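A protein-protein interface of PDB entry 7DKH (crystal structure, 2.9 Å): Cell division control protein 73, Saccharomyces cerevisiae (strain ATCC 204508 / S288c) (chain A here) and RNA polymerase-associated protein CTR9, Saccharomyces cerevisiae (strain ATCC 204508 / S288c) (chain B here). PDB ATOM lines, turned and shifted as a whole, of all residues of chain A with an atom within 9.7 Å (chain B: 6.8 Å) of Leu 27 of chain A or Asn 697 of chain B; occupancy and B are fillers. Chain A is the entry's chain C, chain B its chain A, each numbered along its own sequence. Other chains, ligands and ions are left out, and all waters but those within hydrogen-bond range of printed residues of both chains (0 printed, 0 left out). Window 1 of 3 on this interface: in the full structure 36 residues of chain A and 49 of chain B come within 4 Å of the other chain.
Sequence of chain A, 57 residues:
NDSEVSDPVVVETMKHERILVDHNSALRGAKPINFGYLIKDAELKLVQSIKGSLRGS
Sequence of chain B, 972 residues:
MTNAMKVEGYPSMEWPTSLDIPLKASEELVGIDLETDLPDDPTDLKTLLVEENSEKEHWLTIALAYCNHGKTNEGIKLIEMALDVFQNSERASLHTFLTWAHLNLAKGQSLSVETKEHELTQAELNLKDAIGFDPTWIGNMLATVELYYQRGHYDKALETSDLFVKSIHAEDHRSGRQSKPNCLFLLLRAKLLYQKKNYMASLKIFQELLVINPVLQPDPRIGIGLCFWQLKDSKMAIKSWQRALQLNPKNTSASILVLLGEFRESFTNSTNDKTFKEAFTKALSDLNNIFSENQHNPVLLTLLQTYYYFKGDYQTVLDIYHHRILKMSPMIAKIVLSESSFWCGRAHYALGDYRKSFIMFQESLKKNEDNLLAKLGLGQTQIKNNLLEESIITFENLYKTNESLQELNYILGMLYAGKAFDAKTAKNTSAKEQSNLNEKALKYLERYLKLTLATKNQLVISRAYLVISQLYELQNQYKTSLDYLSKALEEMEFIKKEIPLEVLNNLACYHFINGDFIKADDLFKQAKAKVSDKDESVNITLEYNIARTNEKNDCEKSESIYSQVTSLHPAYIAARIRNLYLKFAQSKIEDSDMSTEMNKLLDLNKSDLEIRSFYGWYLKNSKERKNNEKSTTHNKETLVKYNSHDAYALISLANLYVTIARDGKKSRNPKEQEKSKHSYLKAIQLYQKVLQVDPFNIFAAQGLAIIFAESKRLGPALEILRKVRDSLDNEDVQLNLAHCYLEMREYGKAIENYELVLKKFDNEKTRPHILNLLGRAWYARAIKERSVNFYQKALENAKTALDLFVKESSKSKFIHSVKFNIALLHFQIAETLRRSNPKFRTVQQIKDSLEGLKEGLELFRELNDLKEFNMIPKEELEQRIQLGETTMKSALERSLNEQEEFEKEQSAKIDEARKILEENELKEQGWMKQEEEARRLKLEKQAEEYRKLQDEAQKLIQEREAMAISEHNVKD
Of the 17 printed residues of chain B, 13 touch a printed residue of chain A.
Hydrophobic or aromatic side chains of chain B within 4 Å of the printed part of chain A: Ala 647, Tyr 648, Ile 651, Leu 691, Pro 695, Phe 696, Ile 698, Phe 699, Ala 701 and Val 724.
Among the printed residues, 31 pairs touch across the chains.
The backbone NH of Ile 698 of chain B sits at hydrogen-bond distance from the backbone carbonyl oxygen of Leu 27 of chain A, 2.8 Å away.
The backbone carbonyl oxygen of Pro 695 of chain B sits at hydrogen-bond distance from the backbone NH of Phe 35 of chain A (2.6 Å).
The backbone NH (N) of Tyr 648 of chain B is in hydrogen-bond range of the side-chain amide oxygen (OD1) of Asn 24 of chain A.
The backbone carbonyl oxygen (O) of Ser 727 of chain B lies within hydrogen-bond range of the backbone NH (N) of Ala 30 of chain A, 2.8 Å away.
O of Arg 28 of chain A is in hydrogen-bond range of OG of Ser 727 of chain B, at 3.4 Å.
The side-chain hydroxyl of Ser 727 of chain B is in hydrogen-bond range of the backbone carbonyl oxygen of Lys 31 of chain A.
The side-chain carboxylate of Asp 694 of chain B lies within salt-bridge range of the guanidinium group of Arg 28 of chain A (3.2 Å).
N of Ala 647 of chain B lies within hydrogen-bond range of OD1 of Asn 24 of chain A (3.3 Å).
Asp 22 of chain A touches none of the printed residues of chain B.
Printed residues of chain B within 4 Å of Arg 28 of chain A: Asp 694, Phe 696, Ile 698 and Ser 727.
Printed residues of chain A within 4 Å of Asp 694 of chain B: Arg 28 (3.2 Å).
Asn 697 of chain B touches one residue of chain A.
Of chain A, only Leu 27, Arg 28, Gly 29 and Phe 35 come within 4 Å of Ile 698 of chain B.
The nearest residue of chain A that does not touch Asn 697 of chain B is Asn 24 of chain A (4.3 Å).
Among the printed residues, pairs that only touch across the chains: Gly 29 of chain A with Ser 727 of chain B (3.2 Å), Arg 28 of chain A with Phe 696 of chain B (3.2 Å), Leu 27 of chain A with Asn 697 of chain B (3.3 Å), Ile 33 of chain A with Phe 696 of chain B (3.4 Å), Phe 35 of chain A with Ala 701 of chain B (3.4 Å), Ile 33 of chain A with Ser 727 of chain B (3.4 Å), Phe 35 of chain A with Leu 691 of chain B (3.5 Å), Arg 28 of chain A with Ile 698 of chain B (3.6 Å), Gly 29 of chain A with Ile 698 of chain B (3.6 Å), His 23 of chain A with Tyr 648 of chain B (3.6 Å), Ile 39 of chain A with Leu 691 of chain B (3.6 Å), Asn 34 of chain A with Phe 696 of chain B (3.6 Å), Asn 34 of chain A with Pro 695 of chain B (3.6 Å), Phe 35 of chain A with Val 724 of chain B (3.7 Å), Ile 33 of chain A with Pro 695 of chain B (3.7 Å), Gly 36 of chain A with Pro 695 of chain B (3.7 Å), Leu 27 of chain A with Phe 696 of chain B (3.7 Å), Leu 27 of chain A with Phe 699 of chain B (3.7 Å), Leu 38 of chain A with Ala 701 of chain B (3.7 Å), Pro 32 of chain A with Phe 696 of chain B (3.8 Å), Phe 35 of chain A with Ile 698 of chain B (3.9 Å), Leu 27 of chain A with Ile 651 of chain B (3.9 Å) and Leu 38 of chain A with Leu 691 of chain B (3.999 Å).
The side-chain amide oxygen of Asn 697 of chain B sits close to the backbone NH of Phe 699 of chain B (3.3 Å).
OD1 of Asp 694 of chain B lies close to N of Phe 696 of chain B (3.1 Å).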
ATOM      1  N   VAL A  21     -10.377 -13.591   3.611  1.00  0.00           N
ATOM      2  CA  VAL A  21      -9.086 -14.258   3.728  1.00  0.00           C
ATOM      3  C   VAL A  21      -9.094 -15.447   2.784  1.00  0.00           C
ATOM      4  O   VAL A  21     -10.061 -16.217   2.762  1.00  0.00           O
ATOM      5  CB  VAL A  21      -8.825 -14.746   5.168  1.00  0.00           C
ATOM      6  CG1 VAL A  21      -7.574 -15.603   5.225  1.00  0.00           C
ATOM      7  CG2 VAL A  21      -8.732 -13.576   6.133  1.00  0.00           C
ATOM      8  N   ASP A  22      -8.023 -15.603   2.003  1.00  0.00           N
ATOM      9  CA  ASP A  22      -7.884 -16.767   1.142  1.00  0.00           C
ATOM     10  C   ASP A  22      -6.803 -17.701   1.692  1.00  0.00           C
ATOM     11  O   ASP A  22      -6.236 -17.465   2.765  1.00  0.00           O
ATOM     12  CB  ASP A  22      -7.618 -16.333  -0.310  1.00  0.00           C
ATOM     13  CG  ASP A  22      -6.280 -15.640  -0.498  1.00  0.00           C
ATOM     14  OD1 ASP A  22      -5.522 -15.454   0.484  1.00  0.00           O
ATOM     15  OD2 ASP A  22      -5.989 -15.263  -1.649  1.00  0.00           O
ATOM     16  N   HIS A  23      -6.528 -18.780   0.958  1.00  0.00           N
ATOM     17  CA  HIS A  23      -5.578 -19.779   1.430  1.00  0.00           C
ATOM     18  C   HIS A  23      -4.164 -19.234   1.542  1.00  0.00           C
ATOM     19  O   HIS A  23      -3.345 -19.811   2.260  1.00  0.00           O
ATOM     20  CB  HIS A  23      -5.591 -20.994   0.505  1.00  0.00           C
ATOM     21  CG  HIS A  23      -5.091 -20.709  -0.875  1.00  0.00           C
ATOM     22  ND1 HIS A  23      -5.805 -19.958  -1.782  1.00  0.00           N
ATOM     23  CD2 HIS A  23      -3.945 -21.067  -1.501  1.00  0.00           C
ATOM     24  CE1 HIS A  23      -5.122 -19.869  -2.909  1.00  0.00           C
ATOM     25  NE2 HIS A  23      -3.991 -20.534  -2.767  1.00  0.00           N
ATOM     26  N   ASN A  24      -3.869 -18.142   0.853  1.00  0.00           N
ATOM     27  CA  ASN A  24      -2.547 -17.538   0.828  1.00  0.00           C
ATOM     28  C   ASN A  24      -2.374 -16.406   1.833  1.00  0.00           C
ATOM     29  O   ASN A  24      -1.333 -16.338   2.493  1.00  0.00           O
ATOM     30  CB  ASN A  24      -2.257 -17.023  -0.589  1.00  0.00           C
ATOM     31  CG  ASN A  24      -1.713 -18.102  -1.512  1.00  0.00           C
ATOM     32  OD1 ASN A  24      -0.978 -18.990  -1.083  1.00  0.00           O
ATOM     33  ND2 ASN A  24      -2.091 -18.039  -2.784  1.00  0.00           N
ATOM     34  N   SER A  25      -3.370 -15.523   1.984  1.00  0.00           N
ATOM     35  CA  SER A  25      -3.274 -14.458   2.981  1.00  0.00           C
ATOM     36  C   SER A  25      -3.408 -14.990   4.399  1.00  0.00           C
ATOM     37  O   SER A  25      -2.927 -14.353   5.341  1.00  0.00           O
ATOM     38  CB  SER A  25      -4.329 -13.379   2.721  1.00  0.00           C
ATOM     39  OG  SER A  25      -5.591 -13.949   2.432  1.00  0.00           O
ATOM     40  N   ALA A  26      -4.083 -16.132   4.572  1.00  0.00           N
ATOM     41  CA  ALA A  26      -4.212 -16.744   5.890  1.00  0.00           C
ATOM     42  C   ALA A  26      -2.862 -17.088   6.494  1.00  0.00           C
ATOM     43  O   ALA A  26      -2.778 -17.311   7.707  1.00  0.00           O
ATOM     44  CB  ALA A  26      -5.070 -18.003   5.814  1.00  0.00           C
ATOM     45  N   LEU A  27      -1.810 -17.142   5.676  1.00  0.00           N
ATOM     46  CA  LEU A  27      -0.462 -17.435   6.138  1.00  0.00           C
ATOM     47  C   LEU A  27       0.270 -16.196   6.643  1.00  0.00           C
ATOM     48  O   LEU A  27       1.476 -16.271   6.906  1.00  0.00           O
ATOM     49  CB  LEU A  27       0.328 -18.105   5.007  1.00  0.00           C
ATOM     50  CG  LEU A  27      -0.487 -19.190   4.281  1.00  0.00           C
ATOM     51  CD1 LEU A  27       0.234 -19.751   3.071  1.00  0.00           C
ATOM     52  CD2 LEU A  27      -0.839 -20.327   5.221  1.00  0.00           C
ATOM     53  N   ARG A  28      -0.428 -15.068   6.791  1.00  0.00           N
ATOM     54  CA  ARG A  28       0.131 -13.899   7.457  1.00  0.00           C
ATOM     55  C   ARG A  28      -0.123 -13.918   8.958  1.00  0.00           C
ATOM     56  O   ARG A  28       0.376 -13.041   9.670  1.00  0.00           O
ATOM     57  CB  ARG A  28      -0.433 -12.602   6.854  1.00  0.00           C
ATOM     58  CG  ARG A  28      -0.002 -12.340   5.410  1.00  0.00           C
ATOM     59  CD  ARG A  28      -0.985 -11.458   4.637  1.00  0.00           C
ATOM     60  NE  ARG A  28      -0.330 -10.693   3.576  1.00  0.00           N
ATOM     61  CZ  ARG A  28      -0.252  -9.364   3.532  1.00  0.00           C
ATOM     62  NH1 ARG A  28      -0.800  -8.624   4.489  1.00  0.00           N
ATOM     63  NH2 ARG A  28       0.376  -8.767   2.524  1.00  0.00           N
ATOM     64  N   GLY A  29      -0.904 -14.883   9.449  1.00  0.00           N
ATOM     65  CA  GLY A  29      -1.245 -14.934  10.855  1.00  0.00           C
ATOM     66  C   GLY A  29      -2.352 -13.966  11.235  1.00  0.00           C
ATOM     67  O   GLY A  29      -3.117 -13.465  10.403  1.00  0.00           O
ATOM     68  N   ALA A  30      -2.426 -13.704  12.538  1.00  0.00           N
ATOM     69  CA  ALA A  30      -3.413 -12.780  13.074  1.00  0.00           C
ATOM     70  C   ALA A  30      -2.897 -11.354  13.188  1.00  0.00           C
ATOM     71  O   ALA A  30      -3.700 -10.418  13.137  1.00  0.00           O
ATOM     72  CB  ALA A  30      -3.889 -13.260  14.448  1.00  0.00           C
ATOM     73  N   LYS A  31      -1.588 -11.159  13.340  1.00  0.00           N
ATOM     74  CA  LYS A  31      -0.993  -9.831  13.298  1.00  0.00           C
ATOM     75  C   LYS A  31       0.175  -9.804  12.317  1.00  0.00           C
ATOM     76  O   LYS A  31       0.930 -10.777  12.222  1.00  0.00           O
ATOM     77  CB  LYS A  31      -0.512  -9.375  14.689  1.00  0.00           C
ATOM     78  CG  LYS A  31      -1.338  -9.897  15.855  1.00  0.00           C
ATOM     79  CD  LYS A  31      -1.223  -8.961  17.047  1.00  0.00           C
ATOM     80  CE  LYS A  31      -2.080  -9.410  18.220  1.00  0.00           C
ATOM     81  NZ  LYS A  31      -1.827  -8.554  19.413  1.00  0.00           N
ATOM     82  N   PRO A  32       0.326  -8.721  11.553  1.00  0.00           N
ATOM     83  CA  PRO A  32       1.353  -8.676  10.498  1.00  0.00           C
ATOM     84  C   PRO A  32       2.758  -8.527  11.064  1.00  0.00           C
ATOM     85  O   PRO A  32       3.048  -7.571  11.787  1.00  0.00           O
ATOM     86  CB  PRO A  32       0.945  -7.455   9.665  1.00  0.00           C
ATOM     87  CG  PRO A  32       0.163  -6.601  10.597  1.00  0.00           C
ATOM     88  CD  PRO A  32      -0.527  -7.521  11.558  1.00  0.00           C
ATOM     89  N   ILE A  33       3.626  -9.493  10.760  1.00  0.00           N
ATOM     90  CA  ILE A  33       5.063  -9.379  11.011  1.00  0.00           C
ATOM     91  C   ILE A  33       5.791  -9.449   9.675  1.00  0.00           C
ATOM     92  O   ILE A  33       5.663 -10.440   8.945  1.00  0.00           O
ATOM     93  CB  ILE A  33       5.597 -10.466  11.960  1.00  0.00           C
ATOM     94  CG1 ILE A  33       5.206 -10.184  13.412  1.00  0.00           C
ATOM     95  CG2 ILE A  33       7.103 -10.497  11.888  1.00  0.00           C
ATOM     96  CD1 ILE A  33       3.829 -10.627  13.776  1.00  0.00           C
ATOM     97  N   ASN A  34       6.548  -8.401   9.353  1.00  0.00           N
ATOM     98  CA  ASN A  34       7.353  -8.387   8.136  1.00  0.00           C
ATOM     99  C   ASN A  34       8.590  -9.245   8.366  1.00  0.00           C
ATOM    100  O   ASN A  34       9.462  -8.889   9.165  1.00  0.00           O
ATOM    101  CB  ASN A  34       7.741  -6.960   7.759  1.00  0.00           C
ATOM    102  CG  ASN A  34       8.522  -6.888   6.455  1.00  0.00           C
ATOM    103  OD1 ASN A  34       9.666  -7.344   6.368  1.00  0.00           O
ATOM    104  ND2 ASN A  34       7.912  -6.289   5.440  1.00  0.00           N
ATOM    105  N   PHE A  35       8.669 -10.375   7.663  1.00  0.00           N
ATOM    106  CA  PHE A  35       9.800 -11.285   7.760  1.00  0.00           C
ATOM    107  C   PHE A  35      10.728 -11.187   6.553  1.00  0.00           C
ATOM    108  O   PHE A  35      11.503 -12.116   6.306  1.00  0.00           O
ATOM    109  CB  PHE A  35       9.306 -12.724   7.919  1.00  0.00           C
ATOM    110  CG  PHE A  35       8.897 -13.084   9.320  1.00  0.00           C
ATOM    111  CD1 PHE A  35       9.830 -13.138  10.344  1.00  0.00           C
ATOM    112  CD2 PHE A  35       7.574 -13.388   9.609  1.00  0.00           C
ATOM    113  CE1 PHE A  35       9.450 -13.480  11.634  1.00  0.00           C
ATOM    114  CE2 PHE A  35       7.189 -13.735  10.892  1.00  0.00           C
ATOM    115  CZ  PHE A  35       8.129 -13.778  11.905  1.00  0.00           C
ATOM    116  N   GLY A  36      10.660 -10.092   5.791  1.00  0.00           N
ATOM    117  CA  GLY A  36      11.491  -9.973   4.603  1.00  0.00           C
ATOM    118  C   GLY A  36      12.980 -10.044   4.874  1.00  0.00           C
ATOM    119  O   GLY A  36      13.738 -10.573   4.052  1.00  0.00           O
ATOM    120  N   TYR A  37      13.420  -9.542   6.032  1.00  0.00           N
ATOM    121  CA  TYR A  37      14.839  -9.559   6.370  1.00  0.00           C
ATOM    122  C   TYR A  37      15.421 -10.966   6.342  1.00  0.00           C
ATOM    123  O   TYR A  37      16.621 -11.125   6.077  1.00  0.00           O
ATOM    124  CB  TYR A  37      15.049  -8.923   7.748  1.00  0.00           C
ATOM    125  CG  TYR A  37      14.589  -9.788   8.908  1.00  0.00           C
ATOM    126  CD1 TYR A  37      13.238  -9.907   9.212  1.00  0.00           C
ATOM    127  CD2 TYR A  37      15.500 -10.465   9.711  1.00  0.00           C
ATOM    128  CE1 TYR A  37      12.804 -10.691  10.269  1.00  0.00           C
ATOM    129  CE2 TYR A  37      15.073 -11.248  10.773  1.00  0.00           C
ATOM    130  CZ  TYR A  37      13.725 -11.357  11.045  1.00  0.00           C
ATOM    131  OH  TYR A  37      13.301 -12.135  12.096  1.00  0.00           O
ATOM    132  N   LEU A  38      14.577 -11.993   6.505  1.00  0.00           N
ATOM    133  CA  LEU A  38      15.083 -13.359   6.541  1.00  0.00           C
ATOM    134  C   LEU A  38      15.625 -13.772   5.185  1.00  0.00           C
ATOM    135  O   LEU A  38      16.573 -14.565   5.119  1.00  0.00           O
ATOM    136  CB  LEU A  38      13.980 -14.322   6.980  1.00  0.00           C
ATOM    137  CG  LEU A  38      13.548 -14.249   8.449  1.00  0.00           C
ATOM    138  CD1 LEU A  38      12.488 -15.295   8.770  1.00  0.00           C
ATOM    139  CD2 LEU A  38      14.763 -14.425   9.338  1.00  0.00           C
ATOM    140  N   ILE A  39      15.080 -13.203   4.103  1.00  0.00           N
ATOM    141  CA  ILE A  39      15.637 -13.464   2.778  1.00  0.00           C
ATOM    142  C   ILE A  39      17.138 -13.224   2.802  1.00  0.00           C
ATOM    143  O   ILE A  39      17.922 -14.017   2.267  1.00  0.00           O
ATOM    144  CB  ILE A  39      14.945 -12.595   1.710  1.00  0.00           C
ATOM    145  CG1 ILE A  39      13.421 -12.740   1.780  1.00  0.00           C
ATOM    146  CG2 ILE A  39      15.436 -12.974   0.325  1.00  0.00           C
ATOM    147  CD1 ILE A  39      12.691 -11.958   0.701  1.00  0.00           C
ATOM    148  N   ALA B 647       1.960 -19.105  -2.549  1.00  0.00           N
ATOM    149  CA  ALA B 647       2.691 -19.361  -1.312  1.00  0.00           C
ATOM    150  C   ALA B 647       2.382 -20.742  -0.747  1.00  0.00           C
ATOM    151  O   ALA B 647       3.269 -21.417  -0.221  1.00  0.00           O
ATOM    152  CB  ALA B 647       2.361 -18.279  -0.287  1.00  0.00           C
ATOM    153  N   TYR B 648       1.124 -21.175  -0.843  1.00  0.00           N
ATOM    154  CA  TYR B 648       0.728 -22.451  -0.252  1.00  0.00           C
ATOM    155  C   TYR B 648       1.489 -23.621  -0.875  1.00  0.00           C
ATOM    156  O   TYR B 648       2.144 -24.403  -0.166  1.00  0.00           O
ATOM    157  CB  TYR B 648      -0.785 -22.630  -0.406  1.00  0.00           C
ATOM    158  CG  TYR B 648      -1.418 -23.566   0.597  1.00  0.00           C
ATOM    159  CD1 TYR B 648      -1.459 -24.933   0.366  1.00  0.00           C
ATOM    160  CD2 TYR B 648      -1.972 -23.081   1.775  1.00  0.00           C
ATOM    161  CE1 TYR B 648      -2.039 -25.789   1.270  1.00  0.00           C
ATOM    162  CE2 TYR B 648      -2.553 -23.929   2.693  1.00  0.00           C
ATOM    163  CZ  TYR B 648      -2.583 -25.284   2.434  1.00  0.00           C
ATOM    164  OH  TYR B 648      -3.159 -26.142   3.339  1.00  0.00           O
ATOM    165  N   ALA B 649       1.443 -23.736  -2.206  1.00  0.00           N
ATOM    166  CA  ALA B 649       2.145 -24.824  -2.880  1.00  0.00           C
ATOM    167  C   ALA B 649       3.650 -24.737  -2.663  1.00  0.00           C
ATOM    168  O   ALA B 649       4.318 -25.761  -2.466  1.00  0.00           O
ATOM    169  CB  ALA B 649       1.818 -24.816  -4.372  1.00  0.00           C
ATOM    170  N   ILE B 651       5.243 -23.502  -0.075  1.00  0.00           N
ATOM    171  CA  ILE B 651       5.585 -23.909   1.284  1.00  0.00           C
ATOM    172  C   ILE B 651       5.441 -25.416   1.451  1.00  0.00           C
ATOM    173  O   ILE B 651       6.237 -26.048   2.157  1.00  0.00           O
ATOM    174  CB  ILE B 651       4.730 -23.148   2.312  1.00  0.00           C
ATOM    175  CG1 ILE B 651       5.005 -21.648   2.230  1.00  0.00           C
ATOM    176  CG2 ILE B 651       5.039 -23.632   3.720  1.00  0.00           C
ATOM    177  CD1 ILE B 651       3.999 -20.815   2.982  1.00  0.00           C
ATOM    178  N   VAL B 690       8.744 -17.403  -1.501  1.00  0.00           N
ATOM    179  CA  VAL B 690       7.499 -17.058  -0.818  1.00  0.00           C
ATOM    180  C   VAL B 690       7.625 -15.702  -0.138  1.00  0.00           C
ATOM    181  O   VAL B 690       6.706 -14.874  -0.189  1.00  0.00           O
ATOM    182  CB  VAL B 690       7.145 -18.150   0.206  1.00  0.00           C
ATOM    183  CG1 VAL B 690       5.925 -17.754   1.020  1.00  0.00           C
ATOM    184  CG2 VAL B 690       6.919 -19.441  -0.491  1.00  0.00           C
ATOM    185  N   LEU B 691       8.778 -15.445   0.485  1.00  0.00           N
ATOM    186  CA  LEU B 691       8.964 -14.166   1.162  1.00  0.00           C
ATOM    187  C   LEU B 691       9.095 -13.022   0.168  1.00  0.00           C
ATOM    188  O   LEU B 691       8.772 -11.873   0.498  1.00  0.00           O
ATOM    189  CB  LEU B 691      10.178 -14.233   2.080  1.00  0.00           C
ATOM    190  CG  LEU B 691       9.872 -14.942   3.403  1.00  0.00           C
ATOM    191  CD1 LEU B 691      11.099 -14.987   4.288  1.00  0.00           C
ATOM    192  CD2 LEU B 691       8.708 -14.273   4.124  1.00  0.00           C
ATOM    193  N   ASP B 694       5.441 -12.470  -0.544  1.00  0.00           N
ATOM    194  CA  ASP B 694       4.726 -12.002   0.642  1.00  0.00           C
ATOM    195  C   ASP B 694       5.688 -12.043   1.814  1.00  0.00           C
ATOM    196  O   ASP B 694       5.925 -13.112   2.396  1.00  0.00           O
ATOM    197  CB  ASP B 694       3.488 -12.849   0.922  1.00  0.00           C
ATOM    198  CG  ASP B 694       2.607 -12.256   2.007  1.00  0.00           C
ATOM    199  OD1 ASP B 694       2.931 -11.160   2.517  1.00  0.00           O
ATOM    200  OD2 ASP B 694       1.590 -12.887   2.359  1.00  0.00           O
ATOM    201  N   PRO B 695       6.266 -10.902   2.195  1.00  0.00           N
ATOM    202  CA  PRO B 695       7.186 -10.898   3.341  1.00  0.00           C
ATOM    203  C   PRO B 695       6.483 -11.074   4.681  1.00  0.00           C
ATOM    204  O   PRO B 695       7.166 -11.265   5.697  1.00  0.00           O
ATOM    205  CB  PRO B 695       7.877  -9.536   3.242  1.00  0.00           C
ATOM    206  CG  PRO B 695       7.091  -8.726   2.252  1.00  0.00           C
ATOM    207  CD  PRO B 695       5.976  -9.550   1.694  1.00  0.00           C
ATOM    208  N   PHE B 696       5.151 -11.010   4.716  1.00  0.00           N
ATOM    209  CA  PHE B 696       4.363 -11.224   5.922  1.00  0.00           C
ATOM    210  C   PHE B 696       3.968 -12.689   6.124  1.00  0.00           C
ATOM    211  O   PHE B 696       3.208 -12.994   7.048  1.00  0.00           O
ATOM    212  CB  PHE B 696       3.122 -10.329   5.889  1.00  0.00           C
ATOM    213  CG  PHE B 696       3.441  -8.863   5.965  1.00  0.00           C
ATOM    214  CD1 PHE B 696       3.696  -8.271   7.188  1.00  0.00           C
ATOM    215  CD2 PHE B 696       3.505  -8.082   4.820  1.00  0.00           C
ATOM    216  CE1 PHE B 696       3.998  -6.934   7.277  1.00  0.00           C
ATOM    217  CE2 PHE B 696       3.809  -6.735   4.903  1.00  0.00           C
ATOM    218  CZ  PHE B 696       4.055  -6.163   6.137  1.00  0.00           C
ATOM    219  N   ASN B 697       4.458 -13.592   5.275  1.00  0.00           N
ATOM    220  CA  ASN B 697       4.123 -15.016   5.343  1.00  0.00           C
ATOM    221  C   ASN B 697       4.886 -15.651   6.502  1.00  0.00           C
ATOM    222  O   ASN B 697       6.087 -15.907   6.410  1.00  0.00           O
ATOM    223  CB  ASN B 697       4.446 -15.705   4.021  1.00  0.00           C
ATOM    224  CG  ASN B 697       3.779 -17.066   3.890  1.00  0.00           C
ATOM    225  OD1 ASN B 697       4.105 -17.997   4.623  1.00  0.00           O
ATOM    226  ND2 ASN B 697       2.836 -17.183   2.963  1.00  0.00           N
ATOM    227  N   ILE B 698       4.190 -15.901   7.612  1.00  0.00           N
ATOM    228  CA  ILE B 698       4.871 -16.364   8.815  1.00  0.00           C
ATOM    229  C   ILE B 698       5.195 -17.848   8.759  1.00  0.00           C
ATOM    230  O   ILE B 698       6.046 -18.316   9.526  1.00  0.00           O
ATOM    231  CB  ILE B 698       4.022 -16.067  10.062  1.00  0.00           C
ATOM    232  CG1 ILE B 698       2.826 -17.012  10.114  1.00  0.00           C
ATOM    233  CG2 ILE B 698       3.537 -14.633  10.031  1.00  0.00           C
ATOM    234  CD1 ILE B 698       1.845 -16.702  11.214  1.00  0.00           C
ATOM    235  N   PHE B 699       4.549 -18.602   7.869  1.00  0.00           N
ATOM    236  CA  PHE B 699       4.882 -20.011   7.721  1.00  0.00           C
ATOM    237  C   PHE B 699       6.193 -20.194   6.972  1.00  0.00           C
ATOM    238  O   PHE B 699       6.960 -21.107   7.290  1.00  0.00           O
ATOM    239  CB  PHE B 699       3.744 -20.751   7.015  1.00  0.00           C
ATOM    240  CG  PHE B 699       2.532 -20.965   7.885  1.00  0.00           C
ATOM    241  CD1 PHE B 699       1.582 -19.965   8.023  1.00  0.00           C
ATOM    242  CD2 PHE B 699       2.344 -22.162   8.564  1.00  0.00           C
ATOM    243  CE1 PHE B 699       0.465 -20.149   8.826  1.00  0.00           C
ATOM    244  CE2 PHE B 699       1.227 -22.354   9.368  1.00  0.00           C
ATOM    245  CZ  PHE B 699       0.288 -21.348   9.499  1.00  0.00           C
ATOM    246  N   ALA B 700       6.494 -19.317   6.014  1.00  0.00           N
ATOM    247  CA  ALA B 700       7.826 -19.324   5.419  1.00  0.00           C
ATOM    248  C   ALA B 700       8.884 -19.000   6.464  1.00  0.00           C
ATOM    249  O   ALA B 700       9.949 -19.631   6.505  1.00  0.00           O
ATOM    250  CB  ALA B 700       7.895 -18.331   4.261  1.00  0.00           C
ATOM    251  N   ALA B 701       8.600 -18.024   7.327  1.00  0.00           N
ATOM    252  CA  ALA B 701       9.516 -17.695   8.410  1.00  0.00           C
ATOM    253  C   ALA B 701       9.729 -18.891   9.327  1.00  0.00           C
ATOM    254  O   ALA B 701      10.856 -19.155   9.761  1.00  0.00           O
ATOM    255  CB  ALA B 701       8.981 -16.500   9.196  1.00  0.00           C
ATOM    256  N   GLN B 702       8.653 -19.631   9.632  1.00  0.00           N
ATOM    257  CA  GLN B 702       8.777 -20.785  10.518  1.00  0.00           C
ATOM    258  C   GLN B 702       9.582 -21.905   9.869  1.00  0.00           C
ATOM    259  O   GLN B 702      10.368 -22.578  10.543  1.00  0.00           O
ATOM    260  CB  GLN B 702       7.400 -21.295  10.938  1.00  0.00           C
ATOM    261  CG  GLN B 702       7.450 -22.172  12.185  1.00  0.00           C
ATOM    262  CD  GLN B 702       6.114 -22.797  12.522  1.00  0.00           C
ATOM    263  OE1 GLN B 702       5.791 -23.010  13.689  1.00  0.00           O
ATOM    264  NE2 GLN B 702       5.331 -23.103  11.495  1.00  0.00           N
ATOM    265  N   VAL B 724       7.076 -15.496  15.352  1.00  0.00           N
ATOM    266  CA  VAL B 724       5.958 -16.203  14.735  1.00  0.00           C
ATOM    267  C   VAL B 724       4.853 -16.459  15.753  1.00  0.00           C
ATOM    268  O   VAL B 724       3.662 -16.314  15.448  1.00  0.00           O
ATOM    269  CB  VAL B 724       6.444 -17.511  14.091  1.00  0.00           C
ATOM    270  CG1 VAL B 724       5.256 -18.392  13.723  1.00  0.00           C
ATOM    271  CG2 VAL B 724       7.300 -17.202  12.874  1.00  0.00           C
ATOM    272  N   SER B 727       2.084 -13.990  16.317  1.00  0.00           N
ATOM    273  CA  SER B 727       0.987 -13.828  15.369  1.00  0.00           C
ATOM    274  C   SER B 727       0.350 -15.142  14.943  1.00  0.00           C
ATOM    275  O   SER B 727      -0.468 -15.141  14.015  1.00  0.00           O
ATOM    276  CB  SER B 727       1.455 -13.101  14.116  1.00  0.00           C
ATOM    277  OG  SER B 727       0.709 -13.531  12.992  1.00  0.00           O
